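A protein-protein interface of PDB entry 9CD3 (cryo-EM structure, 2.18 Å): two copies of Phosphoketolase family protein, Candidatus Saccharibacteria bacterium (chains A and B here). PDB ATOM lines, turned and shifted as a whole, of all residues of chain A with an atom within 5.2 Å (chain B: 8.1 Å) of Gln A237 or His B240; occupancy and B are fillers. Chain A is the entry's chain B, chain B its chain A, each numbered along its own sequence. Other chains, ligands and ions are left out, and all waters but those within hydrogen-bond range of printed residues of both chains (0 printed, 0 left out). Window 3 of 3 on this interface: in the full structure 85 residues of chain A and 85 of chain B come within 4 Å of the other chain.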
ATOM      1  N   ASP A 232      20.595 -30.824 -17.552  1.00  0.00           N
ATOM      2  CA  ASP A 232      21.000 -31.371 -18.842  1.00  0.00           C
ATOM      3  C   ASP A 232      20.835 -30.345 -19.954  1.00  0.00           C
ATOM      4  O   ASP A 232      21.675 -30.255 -20.857  1.00  0.00           O
ATOM      5  CB  ASP A 232      20.195 -32.633 -19.156  1.00  0.00           C
ATOM      6  CG  ASP A 232      20.730 -33.857 -18.444  1.00  0.00           C
ATOM      7  OD1 ASP A 232      21.684 -33.717 -17.652  1.00  0.00           O
ATOM      8  OD2 ASP A 232      20.196 -34.961 -18.673  1.00  0.00           O
ATOM      9  N   PHE A 233      19.753 -29.565 -19.909  1.00  0.00           N
ATOM     10  CA  PHE A 233      19.519 -28.554 -20.935  1.00  0.00           C
ATOM     11  C   PHE A 233      20.610 -27.490 -20.927  1.00  0.00           C
ATOM     12  O   PHE A 233      21.066 -27.052 -21.988  1.00  0.00           O
ATOM     13  CB  PHE A 233      18.145 -27.918 -20.733  1.00  0.00           C
ATOM     14  CG  PHE A 233      17.703 -27.057 -21.877  1.00  0.00           C
ATOM     15  CD1 PHE A 233      17.188 -27.625 -23.029  1.00  0.00           C
ATOM     16  CD2 PHE A 233      17.796 -25.678 -21.801  1.00  0.00           C
ATOM     17  CE1 PHE A 233      16.778 -26.835 -24.085  1.00  0.00           C
ATOM     18  CE2 PHE A 233      17.389 -24.884 -22.853  1.00  0.00           C
ATOM     19  CZ  PHE A 233      16.879 -25.463 -23.996  1.00  0.00           C
ATOM     20  N   GLU A 234      21.037 -27.057 -19.739  1.00  0.00           N
ATOM     21  CA  GLU A 234      22.070 -26.029 -19.650  1.00  0.00           C
ATOM     22  C   GLU A 234      23.414 -26.537 -20.156  1.00  0.00           C
ATOM     23  O   GLU A 234      24.141 -25.809 -20.840  1.00  0.00           O
ATOM     24  CB  GLU A 234      22.200 -25.536 -18.209  1.00  0.00           C
ATOM     25  CG  GLU A 234      21.058 -24.661 -17.731  1.00  0.00           C
ATOM     26  CD  GLU A 234      21.355 -24.008 -16.394  1.00  0.00           C
ATOM     27  OE1 GLU A 234      22.026 -22.956 -16.379  1.00  0.00           O
ATOM     28  OE2 GLU A 234      20.921 -24.551 -15.358  1.00  0.00           O
ATOM     29  N   LEU A 235      23.771 -27.777 -19.813  1.00  0.00           N
ATOM     30  CA  LEU A 235      25.079 -28.306 -20.192  1.00  0.00           C
ATOM     31  C   LEU A 235      25.209 -28.430 -21.704  1.00  0.00           C
ATOM     32  O   LEU A 235      26.248 -28.092 -22.279  1.00  0.00           O
ATOM     33  CB  LEU A 235      25.313 -29.660 -19.524  1.00  0.00           C
ATOM     34  CG  LEU A 235      25.618 -29.653 -18.028  1.00  0.00           C
ATOM     35  CD1 LEU A 235      25.252 -30.993 -17.419  1.00  0.00           C
ATOM     36  CD2 LEU A 235      27.074 -29.321 -17.774  1.00  0.00           C
ATOM     37  N   ILE A 236      24.162 -28.927 -22.363  1.00  0.00           N
ATOM     38  CA  ILE A 236      24.202 -29.073 -23.814  1.00  0.00           C
ATOM     39  C   ILE A 236      24.302 -27.710 -24.485  1.00  0.00           C
ATOM     40  O   ILE A 236      25.102 -27.512 -25.406  1.00  0.00           O
ATOM     41  CB  ILE A 236      22.975 -29.863 -24.305  1.00  0.00           C
ATOM     42  CG1 ILE A 236      23.171 -31.359 -24.057  1.00  0.00           C
ATOM     43  CG2 ILE A 236      22.712 -29.597 -25.776  1.00  0.00           C
ATOM     44  CD1 ILE A 236      21.888 -32.151 -24.083  1.00  0.00           C
ATOM     45  N   GLN A 237      23.505 -26.745 -24.020  1.00  0.00           N
ATOM     46  CA  GLN A 237      23.496 -25.421 -24.633  1.00  0.00           C
ATOM     47  C   GLN A 237      24.848 -24.733 -24.498  1.00  0.00           C
ATOM     48  O   GLN A 237      25.315 -24.079 -25.435  1.00  0.00           O
ATOM     49  CB  GLN A 237      22.401 -24.564 -24.004  1.00  0.00           C
ATOM     50  CG  GLN A 237      21.155 -24.423 -24.849  1.00  0.00           C
ATOM     51  CD  GLN A 237      20.213 -23.369 -24.311  1.00  0.00           C
ATOM     52  OE1 GLN A 237      20.379 -22.885 -23.192  1.00  0.00           O
ATOM     53  NE2 GLN A 237      19.216 -23.004 -25.107  1.00  0.00           N
ATOM     54  N   PHE A 238      25.485 -24.860 -23.333  1.00  0.00           N
ATOM     55  CA  PHE A 238      26.753 -24.176 -23.107  1.00  0.00           C
ATOM     56  C   PHE A 238      27.853 -24.733 -24.003  1.00  0.00           C
ATOM     57  O   PHE A 238      28.576 -23.979 -24.663  1.00  0.00           O
ATOM     58  CB  PHE A 238      27.150 -24.287 -21.636  1.00  0.00           C
ATOM     59  CG  PHE A 238      28.515 -23.743 -21.336  1.00  0.00           C
ATOM     60  CD1 PHE A 238      28.699 -22.391 -21.118  1.00  0.00           C
ATOM     61  CD2 PHE A 238      29.612 -24.583 -21.267  1.00  0.00           C
ATOM     62  CE1 PHE A 238      29.950 -21.885 -20.841  1.00  0.00           C
ATOM     63  CE2 PHE A 238      30.866 -24.083 -20.992  1.00  0.00           C
ATOM     64  CZ  PHE A 238      31.035 -22.731 -20.778  1.00  0.00           C
ATOM     65  N   PHE A 239      27.998 -26.059 -24.037  1.00  0.00           N
ATOM     66  CA  PHE A 239      29.088 -26.663 -24.793  1.00  0.00           C
ATOM     67  C   PHE A 239      28.822 -26.653 -26.292  1.00  0.00           C
ATOM     68  O   PHE A 239      29.771 -26.629 -27.082  1.00  0.00           O
ATOM     69  CB  PHE A 239      29.340 -28.087 -24.301  1.00  0.00           C
ATOM     70  CG  PHE A 239      30.094 -28.147 -23.007  1.00  0.00           C
ATOM     71  CD1 PHE A 239      31.396 -27.687 -22.932  1.00  0.00           C
ATOM     72  CD2 PHE A 239      29.498 -28.646 -21.864  1.00  0.00           C
ATOM     73  CE1 PHE A 239      32.092 -27.732 -21.745  1.00  0.00           C
ATOM     74  CE2 PHE A 239      30.191 -28.694 -20.673  1.00  0.00           C
ATOM     75  CZ  PHE A 239      31.489 -28.235 -20.614  1.00  0.00           C
ATOM     76  N   HIS A 240      27.555 -26.668 -26.705  1.00  0.00           N
ATOM     77  CA  HIS A 240      27.250 -26.526 -28.123  1.00  0.00           C
ATOM     78  C   HIS A 240      27.557 -25.127 -28.637  1.00  0.00           C
ATOM     79  O   HIS A 240      27.784 -24.959 -29.839  1.00  0.00           O
ATOM     80  CB  HIS A 240      25.785 -26.868 -28.383  1.00  0.00           C
ATOM     81  CG  HIS A 240      25.498 -27.255 -29.799  1.00  0.00           C
ATOM     82  ND1 HIS A 240      25.549 -26.354 -30.841  1.00  0.00           N
ATOM     83  CD2 HIS A 240      25.159 -28.445 -30.347  1.00  0.00           C
ATOM     84  CE1 HIS A 240      25.252 -26.973 -31.970  1.00  0.00           C
ATOM     85  NE2 HIS A 240      25.012 -28.243 -31.698  1.00  0.00           N
ATOM     86  N   GLY A 241      27.569 -24.126 -27.762  1.00  0.00           N
ATOM     87  CA  GLY A 241      27.894 -22.772 -28.162  1.00  0.00           C
ATOM     88  C   GLY A 241      29.383 -22.506 -28.161  1.00  0.00           C
ATOM     89  O   GLY A 241      29.844 -21.506 -28.718  1.00  0.00           O
ATOM     90  N   LYS B 200      25.839 -17.363  -9.817  1.00  0.00           N
ATOM     91  CA  LYS B 200      25.304 -18.501  -9.082  1.00  0.00           C
ATOM     92  C   LYS B 200      25.664 -18.474  -7.604  1.00  0.00           C
ATOM     93  O   LYS B 200      25.247 -19.369  -6.864  1.00  0.00           O
ATOM     94  CB  LYS B 200      25.798 -19.810  -9.706  1.00  0.00           C
ATOM     95  CG  LYS B 200      25.226 -20.094 -11.081  1.00  0.00           C
ATOM     96  CD  LYS B 200      26.151 -20.983 -11.891  1.00  0.00           C
ATOM     97  CE  LYS B 200      25.415 -21.633 -13.049  1.00  0.00           C
ATOM     98  NZ  LYS B 200      25.980 -21.227 -14.363  1.00  0.00           N
ATOM     99  N   PHE B 233      23.058 -17.288 -33.392  1.00  0.00           N
ATOM    100  CA  PHE B 233      22.611 -18.516 -32.742  1.00  0.00           C
ATOM    101  C   PHE B 233      23.654 -19.020 -31.754  1.00  0.00           C
ATOM    102  O   PHE B 233      23.325 -19.386 -30.619  1.00  0.00           O
ATOM    103  CB  PHE B 233      22.307 -19.576 -33.800  1.00  0.00           C
ATOM    104  CG  PHE B 233      21.608 -20.788 -33.262  1.00  0.00           C
ATOM    105  CD1 PHE B 233      20.244 -20.771 -33.029  1.00  0.00           C
ATOM    106  CD2 PHE B 233      22.313 -21.949 -32.997  1.00  0.00           C
ATOM    107  CE1 PHE B 233      19.597 -21.887 -32.536  1.00  0.00           C
ATOM    108  CE2 PHE B 233      21.672 -23.068 -32.504  1.00  0.00           C
ATOM    109  CZ  PHE B 233      20.313 -23.037 -32.273  1.00  0.00           C
ATOM    110  N   GLU B 234      24.925 -19.030 -32.164  1.00  0.00           N
ATOM    111  CA  GLU B 234      25.989 -19.477 -31.271  1.00  0.00           C
ATOM    112  C   GLU B 234      26.111 -18.574 -30.052  1.00  0.00           C
ATOM    113  O   GLU B 234      26.270 -19.061 -28.928  1.00  0.00           O
ATOM    114  CB  GLU B 234      27.321 -19.533 -32.018  1.00  0.00           C
ATOM    115  CG  GLU B 234      27.476 -20.706 -32.964  1.00  0.00           C
ATOM    116  CD  GLU B 234      28.887 -20.822 -33.510  1.00  0.00           C
ATOM    117  OE1 GLU B 234      29.742 -21.426 -32.828  1.00  0.00           O
ATOM    118  OE2 GLU B 234      29.142 -20.304 -34.616  1.00  0.00           O
ATOM    119  N   LEU B 235      26.048 -17.256 -30.253  1.00  0.00           N
ATOM    120  CA  LEU B 235      26.179 -16.331 -29.130  1.00  0.00           C
ATOM    121  C   LEU B 235      25.041 -16.514 -28.135  1.00  0.00           C
ATOM    122  O   LEU B 235      25.264 -16.567 -26.917  1.00  0.00           O
ATOM    123  CB  LEU B 235      26.220 -14.891 -29.636  1.00  0.00           C
ATOM    124  CG  LEU B 235      27.493 -14.428 -30.342  1.00  0.00           C
ATOM    125  CD1 LEU B 235      27.178 -13.266 -31.264  1.00  0.00           C
ATOM    126  CD2 LEU B 235      28.562 -14.046 -29.338  1.00  0.00           C
ATOM    127  N   ILE B 236      23.809 -16.618 -28.638  1.00  0.00           N
ATOM    128  CA  ILE B 236      22.660 -16.786 -27.757  1.00  0.00           C
ATOM    129  C   ILE B 236      22.749 -18.108 -27.011  1.00  0.00           C
ATOM    130  O   ILE B 236      22.505 -18.169 -25.800  1.00  0.00           O
ATOM    131  CB  ILE B 236      21.349 -16.665 -28.557  1.00  0.00           C
ATOM    132  CG1 ILE B 236      21.008 -15.195 -28.800  1.00  0.00           C
ATOM    133  CG2 ILE B 236      20.207 -17.353 -27.830  1.00  0.00           C
ATOM    134  CD1 ILE B 236      20.046 -14.978 -29.941  1.00  0.00           C
ATOM    135  N   GLN B 237      23.115 -19.185 -27.711  1.00  0.00           N
ATOM    136  CA  GLN B 237      23.223 -20.487 -27.062  1.00  0.00           C
ATOM    137  C   GLN B 237      24.304 -20.485 -25.990  1.00  0.00           C
ATOM    138  O   GLN B 237      24.117 -21.053 -24.909  1.00  0.00           O
ATOM    139  CB  GLN B 237      23.507 -21.567 -28.101  1.00  0.00           C
ATOM    140  CG  GLN B 237      22.322 -22.453 -28.416  1.00  0.00           C
ATOM    141  CD  GLN B 237      22.712 -23.664 -29.235  1.00  0.00           C
ATOM    142  OE1 GLN B 237      23.839 -23.761 -29.720  1.00  0.00           O
ATOM    143  NE2 GLN B 237      21.781 -24.595 -29.395  1.00  0.00           N
ATOM    144  N   PHE B 238      25.447 -19.858 -26.272  1.00  0.00           N
ATOM    145  CA  PHE B 238      26.538 -19.847 -25.306  1.00  0.00           C
ATOM    146  C   PHE B 238      26.177 -19.034 -24.070  1.00  0.00           C
ATOM    147  O   PHE B 238      26.350 -19.500 -22.938  1.00  0.00           O
ATOM    148  CB  PHE B 238      27.809 -19.301 -25.953  1.00  0.00           C
ATOM    149  CG  PHE B 238      28.944 -19.119 -24.990  1.00  0.00           C
ATOM    150  CD1 PHE B 238      29.762 -20.184 -24.660  1.00  0.00           C
ATOM    151  CD2 PHE B 238      29.195 -17.886 -24.415  1.00  0.00           C
ATOM    152  CE1 PHE B 238      30.807 -20.023 -23.775  1.00  0.00           C
ATOM    153  CE2 PHE B 238      30.237 -17.720 -23.527  1.00  0.00           C
ATOM    154  CZ  PHE B 238      31.045 -18.791 -23.208  1.00  0.00           C
ATOM    155  N   PHE B 239      25.679 -17.811 -24.262  1.00  0.00           N
ATOM    156  CA  PHE B 239      25.406 -16.958 -23.113  1.00  0.00           C
ATOM    157  C   PHE B 239      24.155 -17.374 -22.354  1.00  0.00           C
ATOM    158  O   PHE B 239      24.042 -17.073 -21.162  1.00  0.00           O
ATOM    159  CB  PHE B 239      25.311 -15.498 -23.552  1.00  0.00           C
ATOM    160  CG  PHE B 239      26.647 -14.848 -23.740  1.00  0.00           C
ATOM    161  CD1 PHE B 239      27.505 -14.687 -22.667  1.00  0.00           C
ATOM    162  CD2 PHE B 239      27.058 -14.422 -24.989  1.00  0.00           C
ATOM    163  CE1 PHE B 239      28.740 -14.101 -22.834  1.00  0.00           C
ATOM    164  CE2 PHE B 239      28.294 -13.834 -25.161  1.00  0.00           C
ATOM    165  CZ  PHE B 239      29.134 -13.675 -24.081  1.00  0.00           C
ATOM    166  N   HIS B 240      23.218 -18.064 -23.005  1.00  0.00           N
ATOM    167  CA  HIS B 240      22.116 -18.674 -22.275  1.00  0.00           C
ATOM    168  C   HIS B 240      22.553 -19.927 -21.531  1.00  0.00           C
ATOM    169  O   HIS B 240      21.850 -20.367 -20.617  1.00  0.00           O
ATOM    170  CB  HIS B 240      20.973 -19.005 -23.232  1.00  0.00           C
ATOM    171  CG  HIS B 240      19.626 -19.009 -22.582  1.00  0.00           C
ATOM    172  ND1 HIS B 240      19.070 -20.142 -22.029  1.00  0.00           N
ATOM    173  CD2 HIS B 240      18.723 -18.018 -22.398  1.00  0.00           C
ATOM    174  CE1 HIS B 240      17.882 -19.850 -21.533  1.00  0.00           C
ATOM    175  NE2 HIS B 240      17.648 -18.567 -21.742  1.00  0.00           N
ATOM    176  N   GLY B 241      23.693 -20.512 -21.907  1.00  0.00           N
ATOM    177  CA  GLY B 241      24.203 -21.658 -21.173  1.00  0.00           C
ATOM    178  C   GLY B 241      24.615 -21.300 -19.761  1.00  0.00           C
ATOM    179  O   GLY B 241      24.465 -22.102 -18.837  1.00  0.00           O
ATOM    180  N   ALA B 242      25.153 -20.100 -19.576  1.00  0.00           N
ATOM    181  CA  ALA B 242      25.382 -19.564 -18.242  1.00  0.00           C
ATOM    182  C   ALA B 242      24.071 -18.971 -17.727  1.00  0.00           C
ATOM    183  O   ALA B 242      23.009 -19.131 -18.333  1.00  0.00           O
ATOM    184  CB  ALA B 242      26.519 -18.546 -18.267  1.00  0.00           C
ATOM    185  N   GLY B 243      24.126 -18.279 -16.596  1.00  0.00           N
ATOM    186  CA  GLY B 243      22.921 -17.708 -16.026  1.00  0.00           C
ATOM    187  C   GLY B 243      22.661 -16.286 -16.476  1.00  0.00           C
ATOM    188  O   GLY B 243      22.653 -15.365 -15.656  1.00  0.00           O
ATOM    189  N   TRP B 244      22.440 -16.094 -17.774  1.00  0.00           N
ATOM    190  CA  TRP B 244      22.279 -14.761 -18.333  1.00  0.00           C
ATOM    191  C   TRP B 244      21.194 -14.776 -19.398  1.00  0.00           C
ATOM    192  O   TRP B 244      20.828 -15.825 -19.932  1.00  0.00           O
ATOM    193  CB  TRP B 244      23.595 -14.240 -18.918  1.00  0.00           C
ATOM    194  CG  TRP B 244      24.662 -14.084 -17.888  1.00  0.00           C
ATOM    195  CD1 TRP B 244      25.650 -14.974 -17.592  1.00  0.00           C
ATOM    196  CD2 TRP B 244      24.844 -12.974 -17.002  1.00  0.00           C
ATOM    197  NE1 TRP B 244      26.440 -14.485 -16.582  1.00  0.00           N
ATOM    198  CE2 TRP B 244      25.965 -13.258 -16.202  1.00  0.00           C
ATOM    199  CE3 TRP B 244      24.169 -11.766 -16.811  1.00  0.00           C
ATOM    200  CZ2 TRP B 244      26.427 -12.380 -15.227  1.00  0.00           C
ATOM    201  CZ3 TRP B 244      24.629 -10.895 -15.844  1.00  0.00           C
ATOM    202  CH2 TRP B 244      25.746 -11.207 -15.063  1.00  0.00           C
ATOM    203  N   GLU B 245      20.675 -13.586 -19.693  1.00  0.00           N
ATOM    204  CA  GLU B 245      19.627 -13.386 -20.694  1.00  0.00           C
ATOM    205  C   GLU B 245      20.116 -12.325 -21.671  1.00  0.00           C
ATOM    206  O   GLU B 245      19.890 -11.124 -21.469  1.00  0.00           O
ATOM    207  CB  GLU B 245      18.307 -12.982 -20.036  1.00  0.00           C
ATOM    208  CG  GLU B 245      17.256 -14.074 -20.024  1.00  0.00           C
ATOM    209  CD  GLU B 245      16.494 -14.160 -21.329  1.00  0.00           C
ATOM    210  OE1 GLU B 245      16.691 -13.281 -22.193  1.00  0.00           O
ATOM    211  OE2 GLU B 245      15.697 -15.108 -21.492  1.00  0.00           O
ATOM    212  N   PRO B 246      20.796 -12.730 -22.738  1.00  0.00           N
ATOM    213  CA  PRO B 246      21.431 -11.757 -23.628  1.00  0.00           C
ATOM    214  C   PRO B 246      20.489 -11.235 -24.705  1.00  0.00           C
ATOM    215  O   PRO B 246      19.575 -11.919 -25.169  1.00  0.00           O
ATOM    216  CB  PRO B 246      22.579 -12.557 -24.248  1.00  0.00           C
ATOM    217  CG  PRO B 246      22.074 -13.963 -24.272  1.00  0.00           C
ATOM    218  CD  PRO B 246      21.077 -14.118 -23.146  1.00  0.00           C
ATOM    219  N   LYS B 247      20.740  -9.988 -25.097  1.00  0.00           N
ATOM    220  CA  LYS B 247      20.063  -9.341 -26.212  1.00  0.00           C
ATOM    221  C   LYS B 247      21.110  -8.727 -27.131  1.00  0.00           C
ATOM    222  O   LYS B 247      22.139  -8.225 -26.673  1.00  0.00           O
ATOM    223  CB  LYS B 247      19.085  -8.263 -25.734  1.00  0.00           C
ATOM    224  CG  LYS B 247      17.715  -8.333 -26.384  1.00  0.00           C
ATOM    225  CD  LYS B 247      16.972  -9.599 -25.992  1.00  0.00           C
ATOM    226  CE  LYS B 247      16.866  -9.734 -24.481  1.00  0.00           C
ATOM    227  NZ  LYS B 247      15.840 -10.735 -24.081  1.00  0.00           N
ATOM    228  N   ARG B 285      18.067 -15.229 -13.469  1.00  0.00           N
ATOM    229  CA  ARG B 285      18.870 -14.956 -14.655  1.00  0.00           C
ATOM    230  C   ARG B 285      18.857 -13.459 -14.939  1.00  0.00           C
ATOM    231  O   ARG B 285      17.792 -12.877 -15.176  1.00  0.00           O
ATOM    232  CB  ARG B 285      18.343 -15.729 -15.863  1.00  0.00           C
ATOM    233  CG  ARG B 285      17.724 -17.070 -15.523  1.00  0.00           C
ATOM    234  CD  ARG B 285      17.516 -17.903 -16.774  1.00  0.00           C
ATOM    235  NE  ARG B 285      18.707 -17.917 -17.616  1.00  0.00           N
ATOM    236  CZ  ARG B 285      19.471 -18.983 -17.813  1.00  0.00           C
ATOM    237  NH1 ARG B 285      19.191 -20.148 -17.255  1.00  0.00           N
ATOM    238  NH2 ARG B 285      20.545 -18.873 -18.588  1.00  0.00           N
ATOM    239  N   MET B 288      21.790  -9.091 -20.083  1.00  0.00           N
ATOM    240  CA  MET B 288      23.035  -8.518 -20.574  1.00  0.00           C
ATOM    241  C   MET B 288      22.822  -8.066 -22.011  1.00  0.00           C
ATOM    242  O   MET B 288      21.872  -8.484 -22.679  1.00  0.00           O
ATOM    243  CB  MET B 288      24.196  -9.516 -20.470  1.00  0.00           C
ATOM    244  CG  MET B 288      24.025 -10.768 -21.313  1.00  0.00           C
ATOM    245  SD  MET B 288      25.585 -11.472 -21.885  1.00  0.00           S
ATOM    246  CE  MET B 288      26.494  -9.999 -22.338  1.00  0.00           C
ATOM    247  N   ILE B 290      24.594  -7.304 -25.854  1.00  0.00           N
ATOM    248  CA  ILE B 290      25.656  -7.504 -26.835  1.00  0.00           C
ATOM    249  C   ILE B 290      25.485  -6.452 -27.922  1.00  0.00           C
ATOM    250  O   ILE B 290      24.431  -6.381 -28.566  1.00  0.00           O
ATOM    251  CB  ILE B 290      25.626  -8.921 -27.431  1.00  0.00           C
ATOM    252  CG1 ILE B 290      25.854  -9.969 -26.341  1.00  0.00           C
ATOM    253  CG2 ILE B 290      26.670  -9.058 -28.526  1.00  0.00           C
ATOM    254  CD1 ILE B 290      25.193 -11.294 -26.629  1.00  0.00           C
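Hydrophobic or aromatic side chains of chain A that line the printed part of chain B: Phe A238 and His A240. Hydrophobic or aromatic side chains of chain B that line the printed part of chain A: Phe B238 and His B240. Along chain B the printed residues that touch a printed residue of chain A span positions 237 to 241.
ND1 of His A240 lies within hydrogen-bond range of OE1 of Gln B237 (3.3 Å). OE1 of Gln A237 sits at hydrogen-bond distance from ND1 of His B240 (3.3 Å). The backbone carbonyl oxygen of Gln B237 lies close to the backbone carbonyl oxygen of Gln A237 (3.3 Å).
The guanidinium group (NH2) of Arg B285 sits at hydrogen-bond distance from the backbone carbonyl oxygen (O) of His B240 (2.8 Å).
Gln B237 touches its own counterpart, Gln A237. Gln A237 touches His B240, and with the chains exchanged His A240 touches Gln B237. Phe A238 touches its own counterpart, Phe B238. Phe A238 touches Gly B241, but with the chains exchanged Gly A241 does not touch Phe B238 (4.1 Å). Of the 6 pairs that touch across the chains among the printed residues, 4 have their exchanged pair printed and touching as well.
Printed residues of chain B within 4 Å of Glu A234: Gly B241. Gln A237 touches just these residues of chain B: Gln B237 (3.3 Å) and His B240 (3.3 Å). Of the printed residues of chain B, Phe A238 touches Phe B238 and Gly B241. Of the printed residues of chain B, His A240 touches Gln B237 (3.3 Å). Printed residues of chain A within 4 Å of Phe B238: Phe A238 (3.6 Å). His B240 touches just one residue of chain A: Gln A237. The nearest residue of chain A that does not touch His B240 is Glu A234 (5.0 Å). The nearest printed residue of chain A that does not touch Gly B241 is Gln A237 (4.3 Å).
Among the printed residues, merely in contact across the chains: Glu A234 with Gly B241, Phe A238 with Phe B238 and Phe A238 with Gly B241.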
